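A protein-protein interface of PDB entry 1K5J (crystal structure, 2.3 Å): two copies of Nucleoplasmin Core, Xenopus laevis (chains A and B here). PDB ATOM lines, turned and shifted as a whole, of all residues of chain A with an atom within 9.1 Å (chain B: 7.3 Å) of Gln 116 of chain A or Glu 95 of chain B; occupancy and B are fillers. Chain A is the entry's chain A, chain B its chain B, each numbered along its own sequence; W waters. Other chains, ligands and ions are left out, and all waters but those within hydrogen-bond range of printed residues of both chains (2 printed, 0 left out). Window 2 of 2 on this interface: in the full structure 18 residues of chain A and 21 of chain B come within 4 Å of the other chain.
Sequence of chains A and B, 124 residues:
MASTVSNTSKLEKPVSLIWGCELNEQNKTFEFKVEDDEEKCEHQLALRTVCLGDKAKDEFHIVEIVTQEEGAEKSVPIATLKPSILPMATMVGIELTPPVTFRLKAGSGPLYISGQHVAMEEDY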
ATOM      1  N   VAL A  15     -30.130  19.390  19.470  1.00  0.00           N
ATOM      2  CA  VAL A  15     -30.483  19.130  20.901  1.00  0.00           C
ATOM      3  C   VAL A  15     -30.030  20.305  21.784  1.00  0.00           C
ATOM      4  O   VAL A  15     -28.831  20.629  21.869  1.00  0.00           O
ATOM      5  CB  VAL A  15     -29.813  17.832  21.410  1.00  0.00           C
ATOM      6  CG1 VAL A  15     -30.393  17.444  22.776  1.00  0.00           C
ATOM      7  CG2 VAL A  15     -30.016  16.704  20.397  1.00  0.00           C
ATOM      8  N   SER A  16     -31.000  20.951  22.425  1.00  0.00           N
ATOM      9  CA  SER A  16     -30.709  22.083  23.288  1.00  0.00           C
ATOM     10  C   SER A  16     -31.127  21.759  24.721  1.00  0.00           C
ATOM     11  O   SER A  16     -31.886  20.806  24.977  1.00  0.00           O
ATOM     12  CB  SER A  16     -31.442  23.331  22.793  1.00  0.00           C
ATOM     13  OG  SER A  16     -30.709  24.508  23.109  1.00  0.00           O
ATOM     14  N   LEU A  17     -30.622  22.557  25.654  1.00  0.00           N
ATOM     15  CA  LEU A  17     -30.917  22.362  27.064  1.00  0.00           C
ATOM     16  C   LEU A  17     -30.631  23.699  27.770  1.00  0.00           C
ATOM     17  O   LEU A  17     -29.512  24.218  27.678  1.00  0.00           O
ATOM     18  CB  LEU A  17     -29.994  21.264  27.600  1.00  0.00           C
ATOM     19  CG  LEU A  17     -30.338  20.454  28.849  1.00  0.00           C
ATOM     20  CD1 LEU A  17     -31.563  19.564  28.602  1.00  0.00           C
ATOM     21  CD2 LEU A  17     -29.127  19.584  29.188  1.00  0.00           C
ATOM     22  N   ILE A  18     -31.627  24.272  28.450  1.00  0.00           N
ATOM     23  CA  ILE A  18     -31.388  25.534  29.145  1.00  0.00           C
ATOM     24  C   ILE A  18     -30.343  25.269  30.219  1.00  0.00           C
ATOM     25  O   ILE A  18     -30.346  24.217  30.872  1.00  0.00           O
ATOM     26  CB  ILE A  18     -32.669  26.112  29.791  1.00  0.00           C
ATOM     27  CG1 ILE A  18     -32.781  25.676  31.253  1.00  0.00           C
ATOM     28  CG2 ILE A  18     -33.904  25.645  29.017  1.00  0.00           C
ATOM     29  CD1 ILE A  18     -33.973  26.322  31.962  1.00  0.00           C
ATOM     30  N   TRP A  19     -29.446  26.228  30.384  1.00  0.00           N
ATOM     31  CA  TRP A  19     -28.351  26.107  31.337  1.00  0.00           C
ATOM     32  C   TRP A  19     -28.216  27.386  32.172  1.00  0.00           C
ATOM     33  O   TRP A  19     -28.721  28.444  31.800  1.00  0.00           O
ATOM     34  CB  TRP A  19     -27.069  25.836  30.545  1.00  0.00           C
ATOM     35  CG  TRP A  19     -25.783  25.977  31.294  1.00  0.00           C
ATOM     36  CD1 TRP A  19     -25.047  24.975  31.874  1.00  0.00           C
ATOM     37  CD2 TRP A  19     -25.052  27.184  31.499  1.00  0.00           C
ATOM     38  NE1 TRP A  19     -23.895  25.496  32.418  1.00  0.00           N
ATOM     39  CE2 TRP A  19     -23.873  26.852  32.202  1.00  0.00           C
ATOM     40  CE3 TRP A  19     -25.275  28.525  31.149  1.00  0.00           C
ATOM     41  CZ2 TRP A  19     -22.921  27.814  32.571  1.00  0.00           C
ATOM     42  CZ3 TRP A  19     -24.333  29.481  31.511  1.00  0.00           C
ATOM     43  CH2 TRP A  19     -23.166  29.121  32.213  1.00  0.00           C
ATOM     44  N   GLY A  20     -27.527  27.283  33.302  1.00  0.00           N
ATOM     45  CA  GLY A  20     -27.331  28.442  34.144  1.00  0.00           C
ATOM     46  C   GLY A  20     -26.431  28.159  35.323  1.00  0.00           C
ATOM     47  O   GLY A  20     -26.319  27.019  35.757  1.00  0.00           O
ATOM     48  N   PHE A  32     -17.529  25.175  33.126  1.00  0.00           N
ATOM     49  CA  PHE A  32     -18.482  24.406  32.355  1.00  0.00           C
ATOM     50  C   PHE A  32     -17.657  23.379  31.584  1.00  0.00           C
ATOM     51  O   PHE A  32     -16.912  23.734  30.674  1.00  0.00           O
ATOM     52  CB  PHE A  32     -19.232  25.316  31.386  1.00  0.00           C
ATOM     53  CG  PHE A  32     -20.019  24.572  30.343  1.00  0.00           C
ATOM     54  CD1 PHE A  32     -21.073  23.738  30.706  1.00  0.00           C
ATOM     55  CD2 PHE A  32     -19.696  24.700  28.992  1.00  0.00           C
ATOM     56  CE1 PHE A  32     -21.792  23.046  29.739  1.00  0.00           C
ATOM     57  CE2 PHE A  32     -20.409  24.013  28.019  1.00  0.00           C
ATOM     58  CZ  PHE A  32     -21.457  23.186  28.389  1.00  0.00           C
ATOM     59  N   HIS A  43     -20.302  20.061  21.420  1.00  0.00           N
ATOM     60  CA  HIS A  43     -21.095  20.891  22.336  1.00  0.00           C
ATOM     61  C   HIS A  43     -20.778  22.371  22.214  1.00  0.00           C
ATOM     62  O   HIS A  43     -19.637  22.754  21.934  1.00  0.00           O
ATOM     63  CB  HIS A  43     -20.865  20.477  23.793  1.00  0.00           C
ATOM     64  CG  HIS A  43     -21.237  19.055  24.082  1.00  0.00           C
ATOM     65  ND1 HIS A  43     -20.437  17.988  23.733  1.00  0.00           N
ATOM     66  CD2 HIS A  43     -22.338  18.527  24.669  1.00  0.00           C
ATOM     67  CE1 HIS A  43     -21.025  16.862  24.091  1.00  0.00           C
ATOM     68  NE2 HIS A  43     -22.182  17.156  24.662  1.00  0.00           N
ATOM     69  N   GLN A  44     -21.799  23.194  22.427  1.00  0.00           N
ATOM     70  CA  GLN A  44     -21.659  24.645  22.377  1.00  0.00           C
ATOM     71  C   GLN A  44     -22.588  25.256  23.422  1.00  0.00           C
ATOM     72  O   GLN A  44     -23.718  24.790  23.626  1.00  0.00           O
ATOM     73  CB  GLN A  44     -22.010  25.185  20.980  1.00  0.00           C
ATOM     74  N   LEU A  45     -22.088  26.280  24.103  1.00  0.00           N
ATOM     75  CA  LEU A  45     -22.859  26.986  25.114  1.00  0.00           C
ATOM     76  C   LEU A  45     -23.113  28.386  24.588  1.00  0.00           C
ATOM     77  O   LEU A  45     -22.169  29.141  24.372  1.00  0.00           O
ATOM     78  CB  LEU A  45     -22.078  27.100  26.421  1.00  0.00           C
ATOM     79  CG  LEU A  45     -22.894  27.094  27.723  1.00  0.00           C
ATOM     80  CD1 LEU A  45     -22.013  27.582  28.870  1.00  0.00           C
ATOM     81  CD2 LEU A  45     -24.125  27.956  27.588  1.00  0.00           C
ATOM     82  N   ALA A  46     -24.376  28.723  24.363  1.00  0.00           N
ATOM     83  CA  ALA A  46     -24.727  30.058  23.897  1.00  0.00           C
ATOM     84  C   ALA A  46     -25.253  30.815  25.124  1.00  0.00           C
ATOM     85  O   ALA A  46     -26.205  30.375  25.765  1.00  0.00           O
ATOM     86  CB  ALA A  46     -25.805  29.982  22.816  1.00  0.00           C
ATOM     87  N   LEU A  47     -24.615  31.928  25.461  1.00  0.00           N
ATOM     88  CA  LEU A  47     -25.036  32.723  26.613  1.00  0.00           C
ATOM     89  C   LEU A  47     -26.227  33.598  26.254  1.00  0.00           C
ATOM     90  O   LEU A  47     -26.359  34.044  25.112  1.00  0.00           O
ATOM     91  CB  LEU A  47     -23.893  33.611  27.113  1.00  0.00           C
ATOM     92  CG  LEU A  47     -22.617  32.916  27.583  1.00  0.00           C
ATOM     93  CD1 LEU A  47     -21.663  33.956  28.141  1.00  0.00           C
ATOM     94  CD2 LEU A  47     -22.951  31.873  28.619  1.00  0.00           C
ATOM     95  N   ARG A  48     -27.091  33.842  27.234  1.00  0.00           N
ATOM     96  CA  ARG A  48     -28.274  34.666  27.016  1.00  0.00           C
ATOM     97  C   ARG A  48     -28.324  35.899  27.914  1.00  0.00           C
ATOM     98  O   ARG A  48     -28.488  37.018  27.432  1.00  0.00           O
ATOM     99  CB  ARG A  48     -29.538  33.828  27.209  1.00  0.00           C
ATOM    100  CG  ARG A  48     -29.625  32.637  26.275  1.00  0.00           C
ATOM    101  CD  ARG A  48     -29.378  33.048  24.829  1.00  0.00           C
ATOM    102  NE  ARG A  48     -29.582  31.928  23.916  1.00  0.00           N
ATOM    103  CZ  ARG A  48     -29.037  31.836  22.709  1.00  0.00           C
ATOM    104  NH1 ARG A  48     -28.246  32.792  22.252  1.00  0.00           N
ATOM    105  NH2 ARG A  48     -29.281  30.772  21.955  1.00  0.00           N
ATOM    106  N   THR A  49     -28.190  35.697  29.218  1.00  0.00           N
ATOM    107  CA  THR A  49     -28.225  36.824  30.135  1.00  0.00           C
ATOM    108  C   THR A  49     -27.333  36.642  31.351  1.00  0.00           C
ATOM    109  O   THR A  49     -26.944  35.529  31.712  1.00  0.00           O
ATOM    110  CB  THR A  49     -29.657  37.092  30.679  1.00  0.00           C
ATOM    111  OG1 THR A  49     -30.124  35.931  31.371  1.00  0.00           O
ATOM    112  CG2 THR A  49     -30.624  37.436  29.564  1.00  0.00           C
ATOM    113  N   ILE A  94     -22.772  35.061  21.711  1.00  0.00           N
ATOM    114  CA  ILE A  94     -21.637  34.488  22.402  1.00  0.00           C
ATOM    115  C   ILE A  94     -21.834  32.978  22.515  1.00  0.00           C
ATOM    116  O   ILE A  94     -22.628  32.497  23.329  1.00  0.00           O
ATOM    117  CB  ILE A  94     -21.455  35.115  23.794  1.00  0.00           C
ATOM    118  CG1 ILE A  94     -20.986  36.562  23.648  1.00  0.00           C
ATOM    119  CG2 ILE A  94     -20.439  34.324  24.598  1.00  0.00           C
ATOM    120  CD1 ILE A  94     -20.812  37.291  24.970  1.00  0.00           C
ATOM    121  N   GLU A  95     -21.126  32.236  21.670  1.00  0.00           N
ATOM    122  CA  GLU A  95     -21.205  30.779  21.674  1.00  0.00           C
ATOM    123  C   GLU A  95     -19.834  30.221  22.014  1.00  0.00           C
ATOM    124  O   GLU A  95     -18.844  30.529  21.355  1.00  0.00           O
ATOM    125  CB  GLU A  95     -21.671  30.274  20.316  1.00  0.00           C
ATOM    126  CG  GLU A  95     -23.175  30.154  20.232  1.00  0.00           C
ATOM    127  CD  GLU A  95     -23.727  30.671  18.929  1.00  0.00           C
ATOM    128  OE1 GLU A  95     -23.143  30.337  17.868  1.00  0.00           O
ATOM    129  OE2 GLU A  95     -24.743  31.402  18.973  1.00  0.00           O
ATOM    130  N   LEU A  96     -19.782  29.387  23.039  1.00  0.00           N
ATOM    131  CA  LEU A  96     -18.514  28.854  23.500  1.00  0.00           C
ATOM    132  C   LEU A  96     -18.397  27.347  23.397  1.00  0.00           C
ATOM    133  O   LEU A  96     -19.375  26.616  23.543  1.00  0.00           O
ATOM    134  CB  LEU A  96     -18.299  29.282  24.958  1.00  0.00           C
ATOM    135  CG  LEU A  96     -18.528  30.772  25.239  1.00  0.00           C
ATOM    136  CD1 LEU A  96     -18.982  30.969  26.686  1.00  0.00           C
ATOM    137  CD2 LEU A  96     -17.254  31.541  24.943  1.00  0.00           C
ATOM    138  N   PRO A  98     -16.898  24.109  25.076  1.00  0.00           N
ATOM    139  CA  PRO A  98     -16.338  23.683  26.360  1.00  0.00           C
ATOM    140  C   PRO A  98     -14.938  23.123  26.145  1.00  0.00           C
ATOM    141  O   PRO A  98     -14.621  22.641  25.057  1.00  0.00           O
ATOM    142  CB  PRO A  98     -17.327  22.622  26.837  1.00  0.00           C
ATOM    143  CG  PRO A  98     -17.820  22.037  25.555  1.00  0.00           C
ATOM    144  CD  PRO A  98     -18.056  23.277  24.711  1.00  0.00           C
ATOM    145  N   ILE A 113     -25.785  33.479  35.411  1.00  0.00           N
ATOM    146  CA  ILE A 113     -25.478  33.467  33.999  1.00  0.00           C
ATOM    147  C   ILE A 113     -26.416  32.439  33.418  1.00  0.00           C
ATOM    148  O   ILE A 113     -26.505  31.325  33.918  1.00  0.00           O
ATOM    149  CB  ILE A 113     -24.035  33.034  33.718  1.00  0.00           C
ATOM    150  CG1 ILE A 113     -23.059  33.918  34.495  1.00  0.00           C
ATOM    151  CG2 ILE A 113     -23.764  33.128  32.227  1.00  0.00           C
ATOM    152  CD1 ILE A 113     -21.595  33.563  34.265  1.00  0.00           C
ATOM    153  N   SER A 114     -27.150  32.819  32.387  1.00  0.00           N
ATOM    154  CA  SER A 114     -28.074  31.889  31.763  1.00  0.00           C
ATOM    155  C   SER A 114     -27.586  31.614  30.352  1.00  0.00           C
ATOM    156  O   SER A 114     -26.880  32.436  29.755  1.00  0.00           O
ATOM    157  CB  SER A 114     -29.482  32.485  31.704  1.00  0.00           C
ATOM    158  OG  SER A 114     -29.529  33.550  30.775  1.00  0.00           O
ATOM    159  N   GLY A 115     -27.978  30.466  29.815  1.00  0.00           N
ATOM    160  CA  GLY A 115     -27.576  30.119  28.466  1.00  0.00           C
ATOM    161  C   GLY A 115     -28.233  28.852  27.966  1.00  0.00           C
ATOM    162  O   GLY A 115     -29.030  28.224  28.665  1.00  0.00           O
ATOM    163  N   GLN A 116     -27.908  28.485  26.736  1.00  0.00           N
ATOM    164  CA  GLN A 116     -28.451  27.272  26.141  1.00  0.00           C
ATOM    165  C   GLN A 116     -27.296  26.357  25.773  1.00  0.00           C
ATOM    166  O   GLN A 116     -26.392  26.736  25.032  1.00  0.00           O
ATOM    167  CB  GLN A 116     -29.286  27.600  24.901  1.00  0.00           C
ATOM    168  CG  GLN A 116     -30.528  28.438  25.217  1.00  0.00           C
ATOM    169  CD  GLN A 116     -31.317  28.827  23.973  1.00  0.00           C
ATOM    170  OE1 GLN A 116     -32.153  29.732  24.023  1.00  0.00           O
ATOM    171  NE2 GLN A 116     -31.056  28.136  22.847  1.00  0.00           N
ATOM    172  N   HIS A 117     -27.323  25.158  26.327  1.00  0.00           N
ATOM    173  CA  HIS A 117     -26.289  24.180  26.064  1.00  0.00           C
ATOM    174  C   HIS A 117     -26.792  23.268  24.968  1.00  0.00           C
ATOM    175  O   HIS A 117     -27.582  22.375  25.238  1.00  0.00           O
ATOM    176  CB  HIS A 117     -26.011  23.368  27.327  1.00  0.00           C
ATOM    177  CG  HIS A 117     -25.125  22.192  27.095  1.00  0.00           C
ATOM    178  ND1 HIS A 117     -23.949  22.276  26.377  1.00  0.00           N
ATOM    179  CD2 HIS A 117     -25.225  20.905  27.504  1.00  0.00           C
ATOM    180  CE1 HIS A 117     -23.363  21.093  26.355  1.00  0.00           C
ATOM    181  NE2 HIS A 117     -24.116  20.241  27.031  1.00  0.00           N
ATOM    182  N   VAL A 118     -26.341  23.497  23.737  1.00  0.00           N
ATOM    183  CA  VAL A 118     -26.779  22.679  22.601  1.00  0.00           C
ATOM    184  C   VAL A 118     -25.740  21.631  22.191  1.00  0.00           C
ATOM    185  O   VAL A 118     -24.533  21.854  22.325  1.00  0.00           O
ATOM    186  CB  VAL A 118     -27.103  23.559  21.341  1.00  0.00           C
ATOM    187  CG1 VAL A 118     -27.817  24.830  21.757  1.00  0.00           C
ATOM    188  CG2 VAL A 118     -25.825  23.900  20.581  1.00  0.00           C
ATOM    189  N   ALA A 119     -26.216  20.487  21.704  1.00  0.00           N
ATOM    190  CA  ALA A 119     -25.326  19.420  21.239  1.00  0.00           C
ATOM    191  C   ALA A 119     -25.935  18.691  20.026  1.00  0.00           C
ATOM    192  O   ALA A 119     -27.181  18.537  19.992  1.00  0.00           O
ATOM    193  CB  ALA A 119     -25.058  18.424  22.361  1.00  0.00           C
ATOM    194  N   GLN B  44     -42.165  25.926  19.865  1.00  0.00           N
ATOM    195  CA  GLN B  44     -41.055  26.701  20.375  1.00  0.00           C
ATOM    196  C   GLN B  44     -41.577  28.044  20.812  1.00  0.00           C
ATOM    197  O   GLN B  44     -42.469  28.612  20.182  1.00  0.00           O
ATOM    198  CB  GLN B  44     -39.974  26.914  19.321  1.00  0.00           C
ATOM    199  CG  GLN B  44     -38.922  25.824  19.326  1.00  0.00           C
ATOM    200  CD  GLN B  44     -37.569  26.315  18.843  1.00  0.00           C
ATOM    201  OE1 GLN B  44     -36.558  25.605  18.969  1.00  0.00           O
ATOM    202  NE2 GLN B  44     -37.535  27.535  18.290  1.00  0.00           N
ATOM    203  N   LEU B  45     -41.031  28.531  21.914  1.00  0.00           N
ATOM    204  CA  LEU B  45     -41.405  29.837  22.419  1.00  0.00           C
ATOM    205  C   LEU B  45     -40.144  30.678  22.372  1.00  0.00           C
ATOM    206  O   LEU B  45     -39.162  30.350  23.039  1.00  0.00           O
ATOM    207  CB  LEU B  45     -41.882  29.747  23.866  1.00  0.00           C
ATOM    208  CG  LEU B  45     -42.939  30.772  24.299  1.00  0.00           C
ATOM    209  CD1 LEU B  45     -43.007  30.790  25.812  1.00  0.00           C
ATOM    210  CD2 LEU B  45     -42.619  32.149  23.771  1.00  0.00           C
ATOM    211  N   ALA B  46     -40.163  31.739  21.573  1.00  0.00           N
ATOM    212  CA  ALA B  46     -39.026  32.638  21.482  1.00  0.00           C
ATOM    213  C   ALA B  46     -39.383  33.887  22.304  1.00  0.00           C
ATOM    214  O   ALA B  46     -40.376  34.561  22.016  1.00  0.00           O
ATOM    215  CB  ALA B  46     -38.756  33.018  20.027  1.00  0.00           C
ATOM    216  N   LEU B  47     -38.584  34.183  23.326  1.00  0.00           N
ATOM    217  CA  LEU B  47     -38.849  35.338  24.170  1.00  0.00           C
ATOM    218  C   LEU B  47     -38.383  36.612  23.499  1.00  0.00           C
ATOM    219  O   LEU B  47     -37.424  36.596  22.731  1.00  0.00           O
ATOM    220  CB  LEU B  47     -38.160  35.183  25.526  1.00  0.00           C
ATOM    221  CG  LEU B  47     -38.556  33.988  26.385  1.00  0.00           C
ATOM    222  CD1 LEU B  47     -37.837  34.076  27.732  1.00  0.00           C
ATOM    223  CD2 LEU B  47     -40.065  33.968  26.574  1.00  0.00           C
ATOM    224  N   ARG B  48     -39.061  37.719  23.791  1.00  0.00           N
ATOM    225  CA  ARG B  48     -38.707  39.006  23.204  1.00  0.00           C
ATOM    226  C   ARG B  48     -38.399  40.077  24.248  1.00  0.00           C
ATOM    227  O   ARG B  48     -37.357  40.727  24.193  1.00  0.00           O
ATOM    228  CB  ARG B  48     -39.830  39.500  22.285  1.00  0.00           C
ATOM    229  CG  ARG B  48     -40.138  38.554  21.141  1.00  0.00           C
ATOM    230  CD  ARG B  48     -38.865  38.125  20.409  1.00  0.00           C
ATOM    231  NE  ARG B  48     -39.174  37.325  19.231  1.00  0.00           N
ATOM    232  CZ  ARG B  48     -38.328  36.475  18.654  1.00  0.00           C
ATOM    233  NH1 ARG B  48     -37.106  36.304  19.144  1.00  0.00           N
ATOM    234  NH2 ARG B  48     -38.713  35.779  17.587  1.00  0.00           N
ATOM    235  N   VAL B  92     -32.886  37.980  23.789  1.00  0.00           N
ATOM    236  CA  VAL B  92     -32.399  37.629  22.453  1.00  0.00           C
ATOM    237  C   VAL B  92     -31.920  36.194  22.343  1.00  0.00           C
ATOM    238  O   VAL B  92     -31.174  35.713  23.186  1.00  0.00           O
ATOM    239  CB  VAL B  92     -31.230  38.536  22.024  1.00  0.00           C
ATOM    240  CG1 VAL B  92     -30.781  38.164  20.619  1.00  0.00           C
ATOM    241  CG2 VAL B  92     -31.648  39.999  22.089  1.00  0.00           C
ATOM    242  N   GLY B  93     -32.351  35.520  21.285  1.00  0.00           N
ATOM    243  CA  GLY B  93     -31.937  34.148  21.061  1.00  0.00           C
ATOM    244  C   GLY B  93     -32.408  33.146  22.091  1.00  0.00           C
ATOM    245  O   GLY B  93     -31.840  32.066  22.200  1.00  0.00           O
ATOM    246  N   ILE B  94     -33.434  33.473  22.861  1.00  0.00           N
ATOM    247  CA  ILE B  94     -33.921  32.519  23.834  1.00  0.00           C
ATOM    248  C   ILE B  94     -35.149  31.796  23.265  1.00  0.00           C
ATOM    249  O   ILE B  94     -36.251  32.357  23.189  1.00  0.00           O
ATOM    250  CB  ILE B  94     -34.264  33.215  25.162  1.00  0.00           C
ATOM    251  CG1 ILE B  94     -32.975  33.680  25.841  1.00  0.00           C
ATOM    252  CG2 ILE B  94     -35.015  32.270  26.078  1.00  0.00           C
ATOM    253  CD1 ILE B  94     -33.206  34.442  27.138  1.00  0.00           C
ATOM    254  N   GLU B  95     -34.942  30.555  22.840  1.00  0.00           N
ATOM    255  CA  GLU B  95     -36.021  29.745  22.276  1.00  0.00           C
ATOM    256  C   GLU B  95     -36.197  28.525  23.146  1.00  0.00           C
ATOM    257  O   GLU B  95     -35.250  27.779  23.391  1.00  0.00           O
ATOM    258  CB  GLU B  95     -35.695  29.354  20.842  1.00  0.00           C
ATOM    259  CG  GLU B  95     -36.195  30.374  19.845  1.00  0.00           C
ATOM    260  CD  GLU B  95     -35.215  30.641  18.734  1.00  0.00           C
ATOM    261  OE1 GLU B  95     -34.630  29.658  18.225  1.00  0.00           O
ATOM    262  OE2 GLU B  95     -35.039  31.830  18.372  1.00  0.00           O
ATOM    263  N   LEU B  96     -37.419  28.319  23.613  1.00  0.00           N
ATOM    264  CA  LEU B  96     -37.688  27.225  24.522  1.00  0.00           C
ATOM    265  C   LEU B  96     -38.672  26.215  23.990  1.00  0.00           C
ATOM    266  O   LEU B  96     -39.589  26.552  23.244  1.00  0.00           O
ATOM    267  CB  LEU B  96     -38.209  27.808  25.840  1.00  0.00           C
ATOM    268  CG  LEU B  96     -37.375  28.958  26.425  1.00  0.00           C
ATOM    269  CD1 LEU B  96     -38.270  29.881  27.256  1.00  0.00           C
ATOM    270  CD2 LEU B  96     -36.236  28.392  27.258  1.00  0.00           C
ATOM    271  N   THR B  97     -38.477  24.972  24.400  1.00  0.00           N
ATOM    272  CA  THR B  97     -39.340  23.870  24.011  1.00  0.00           C
ATOM    273  C   THR B  97     -40.271  23.595  25.184  1.00  0.00           C
ATOM    274  O   THR B  97     -39.806  23.278  26.283  1.00  0.00           O
ATOM    275  CB  THR B  97     -38.518  22.607  23.733  1.00  0.00           C
ATOM    276  OG1 THR B  97     -37.601  22.870  22.665  1.00  0.00           O
ATOM    277  CG2 THR B  97     -39.420  21.445  23.387  1.00  0.00           C
ATOM    278  N   GLN B 116     -42.879  34.957  21.056  1.00  0.00           N
ATOM    279  CA  GLN B 116     -43.544  34.450  19.868  1.00  0.00           C
ATOM    280  C   GLN B 116     -43.638  32.953  19.976  1.00  0.00           C
ATOM    281  O   GLN B 116     -42.633  32.247  20.103  1.00  0.00           O
ATOM    282  CB  GLN B 116     -42.789  34.838  18.599  1.00  0.00           C
ATOM    283  CG  GLN B 116     -42.776  36.341  18.376  1.00  0.00           C
ATOM    284  CD  GLN B 116     -41.999  36.749  17.144  1.00  0.00           C
ATOM    285  OE1 GLN B 116     -41.645  37.923  16.988  1.00  0.00           O
ATOM    286  NE2 GLN B 116     -41.733  35.784  16.251  1.00  0.00           N
ATOM    287  N   VAL B 118     -44.231  29.834  18.136  1.00  0.00           N
ATOM    288  CA  VAL B 118     -44.278  29.273  16.785  1.00  0.00           C
ATOM    289  C   VAL B 118     -44.499  27.756  16.859  1.00  0.00           C
ATOM    290  O   VAL B 118     -43.861  27.061  17.668  1.00  0.00           O
ATOM    291  CB  VAL B 118     -42.967  29.584  15.979  1.00  0.00           C
ATOM    292  CG1 VAL B 118     -42.354  30.897  16.461  1.00  0.00           C
ATOM    293  CG2 VAL B 118     -41.969  28.440  16.098  1.00  0.00           C
HETATM  294  O   HOH W   1     -31.112  36.878  25.786  1.00  0.00           O
HETATM  295  O   HOH W   2     -28.195  35.461  22.919  1.00  0.00           O
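The side-chain amide oxygen (OE1) of Gln 116 of chain A lies close to the backbone carbonyl oxygen (O) of Gly 93 of chain B, 3.0 Å away.
The side-chain amide oxygen of Gln 116 of chain A is in hydrogen-bond range of the backbone NH of Glu 95 of chain B (3.1 Å).
The guanidinium group of Arg 48 of chain A is in hydrogen-bond range of the backbone carbonyl oxygen of Gly 93 of chain B (2.8 Å).
O of Ala 46 of chain A sits at hydrogen-bond distance from N of Gln 116 of chain A, 2.7 Å away.
The backbone NH of Arg 48 of chain A is in hydrogen-bond range of the backbone carbonyl oxygen of Ser 114 of chain A (2.9 Å).
The backbone carbonyl oxygen of Ile 94 of chain B sits at hydrogen-bond distance from the backbone NH of Leu 47 of chain B (3.0 Å).
The guanidinium group of Arg 48 of chain A sits close to the side-chain amide nitrogen of Gln 116 of chain A (3.3 Å).
Arg 48 of chain A touches Val 92 of chain B.
CG of Arg 48 of chain A touches CG1 of Ile 94 of chain B, at 3.5 Å.
Gln 116 of chain A touches Ile 94 of chain B (OE1 to CA, 3.3 Å).
Of chain B, only Gly 93 (3.0 Å), Ile 94 (3.3 Å) and Glu 95 (3.1 Å) come within 4 Å of Gln 116 of chain A.
Glu 95 of chain B touches just one residue of chain A: Gln 116.
Of the printed residues of chain B, Arg 48 of chain A touches Val 92 (3.6 Å), Gly 93 (2.8 Å) and Ile 94 (3.5 Å).
Printed residues of chain A within 4 Å of Ile 94 of chain B: Arg 48 (3.5 Å) and Gln 116 (3.3 Å).
Printed residues of chain A within 4 Å of Gly 93 of chain B: Arg 48 and Gln 116.
Gly 20 of chain A touches none of the printed residues of chain B.
Thr 49 of chain A touches none of the printed residues of chain B.
The nearest residue of chain A that does not touch Glu 95 of chain B is Ser 16 of chain A (5.6 Å).
The nearest printed residue of chain A that does not touch Ile 94 of chain B is Thr 49 of chain A (4.6 Å).
Of the 25 printed residues of chain A, 2 touch a printed residue of chain B.
Hydrophobic or aromatic side chains of chain B that line the printed part of chain A: Ile 94.
Among the printed residues, 6 pairs touch across the chains.
Among the printed residues, no Asp or Glu carboxylate lies within 4 Å of a Lys or Arg side-chain nitrogen of the other chain.
Arg 48 of chain A touches Ile 94 of chain B, but with the chains exchanged Ile 94 of chain A does not touch Arg 48 of chain B (14.6 Å).
Gln 116 of chain A touches Ile 94 of chain B, but with the chains exchanged Ile 94 of chain A does not touch Gln 116 of chain B (19.7 Å).
Gln 116 of chain A touches Glu 95 of chain B, but with the chains exchanged Glu 95 of chain A does not touch Gln 116 of chain B (17.8 Å).
10 positions are printed for both chains.
Of the 6 pairs that touch across the chains among the printed residues, none has its exchanged pair printed and touching as well.
Water W2 lies within hydrogen-bond range of the guanidinium group (NH1) of Arg 48 of chain A (2.8 Å), the backbone carbonyl oxygen (O) of Val 92 of chain B (3.0 Å) and the backbone carbonyl oxygen (O) of Leu 47 of chain A (3.2 Å).
Water W1 bridges O of Val 92 of chain B (2.8 Å) and O of Arg 48 of chain A (3.1 Å).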
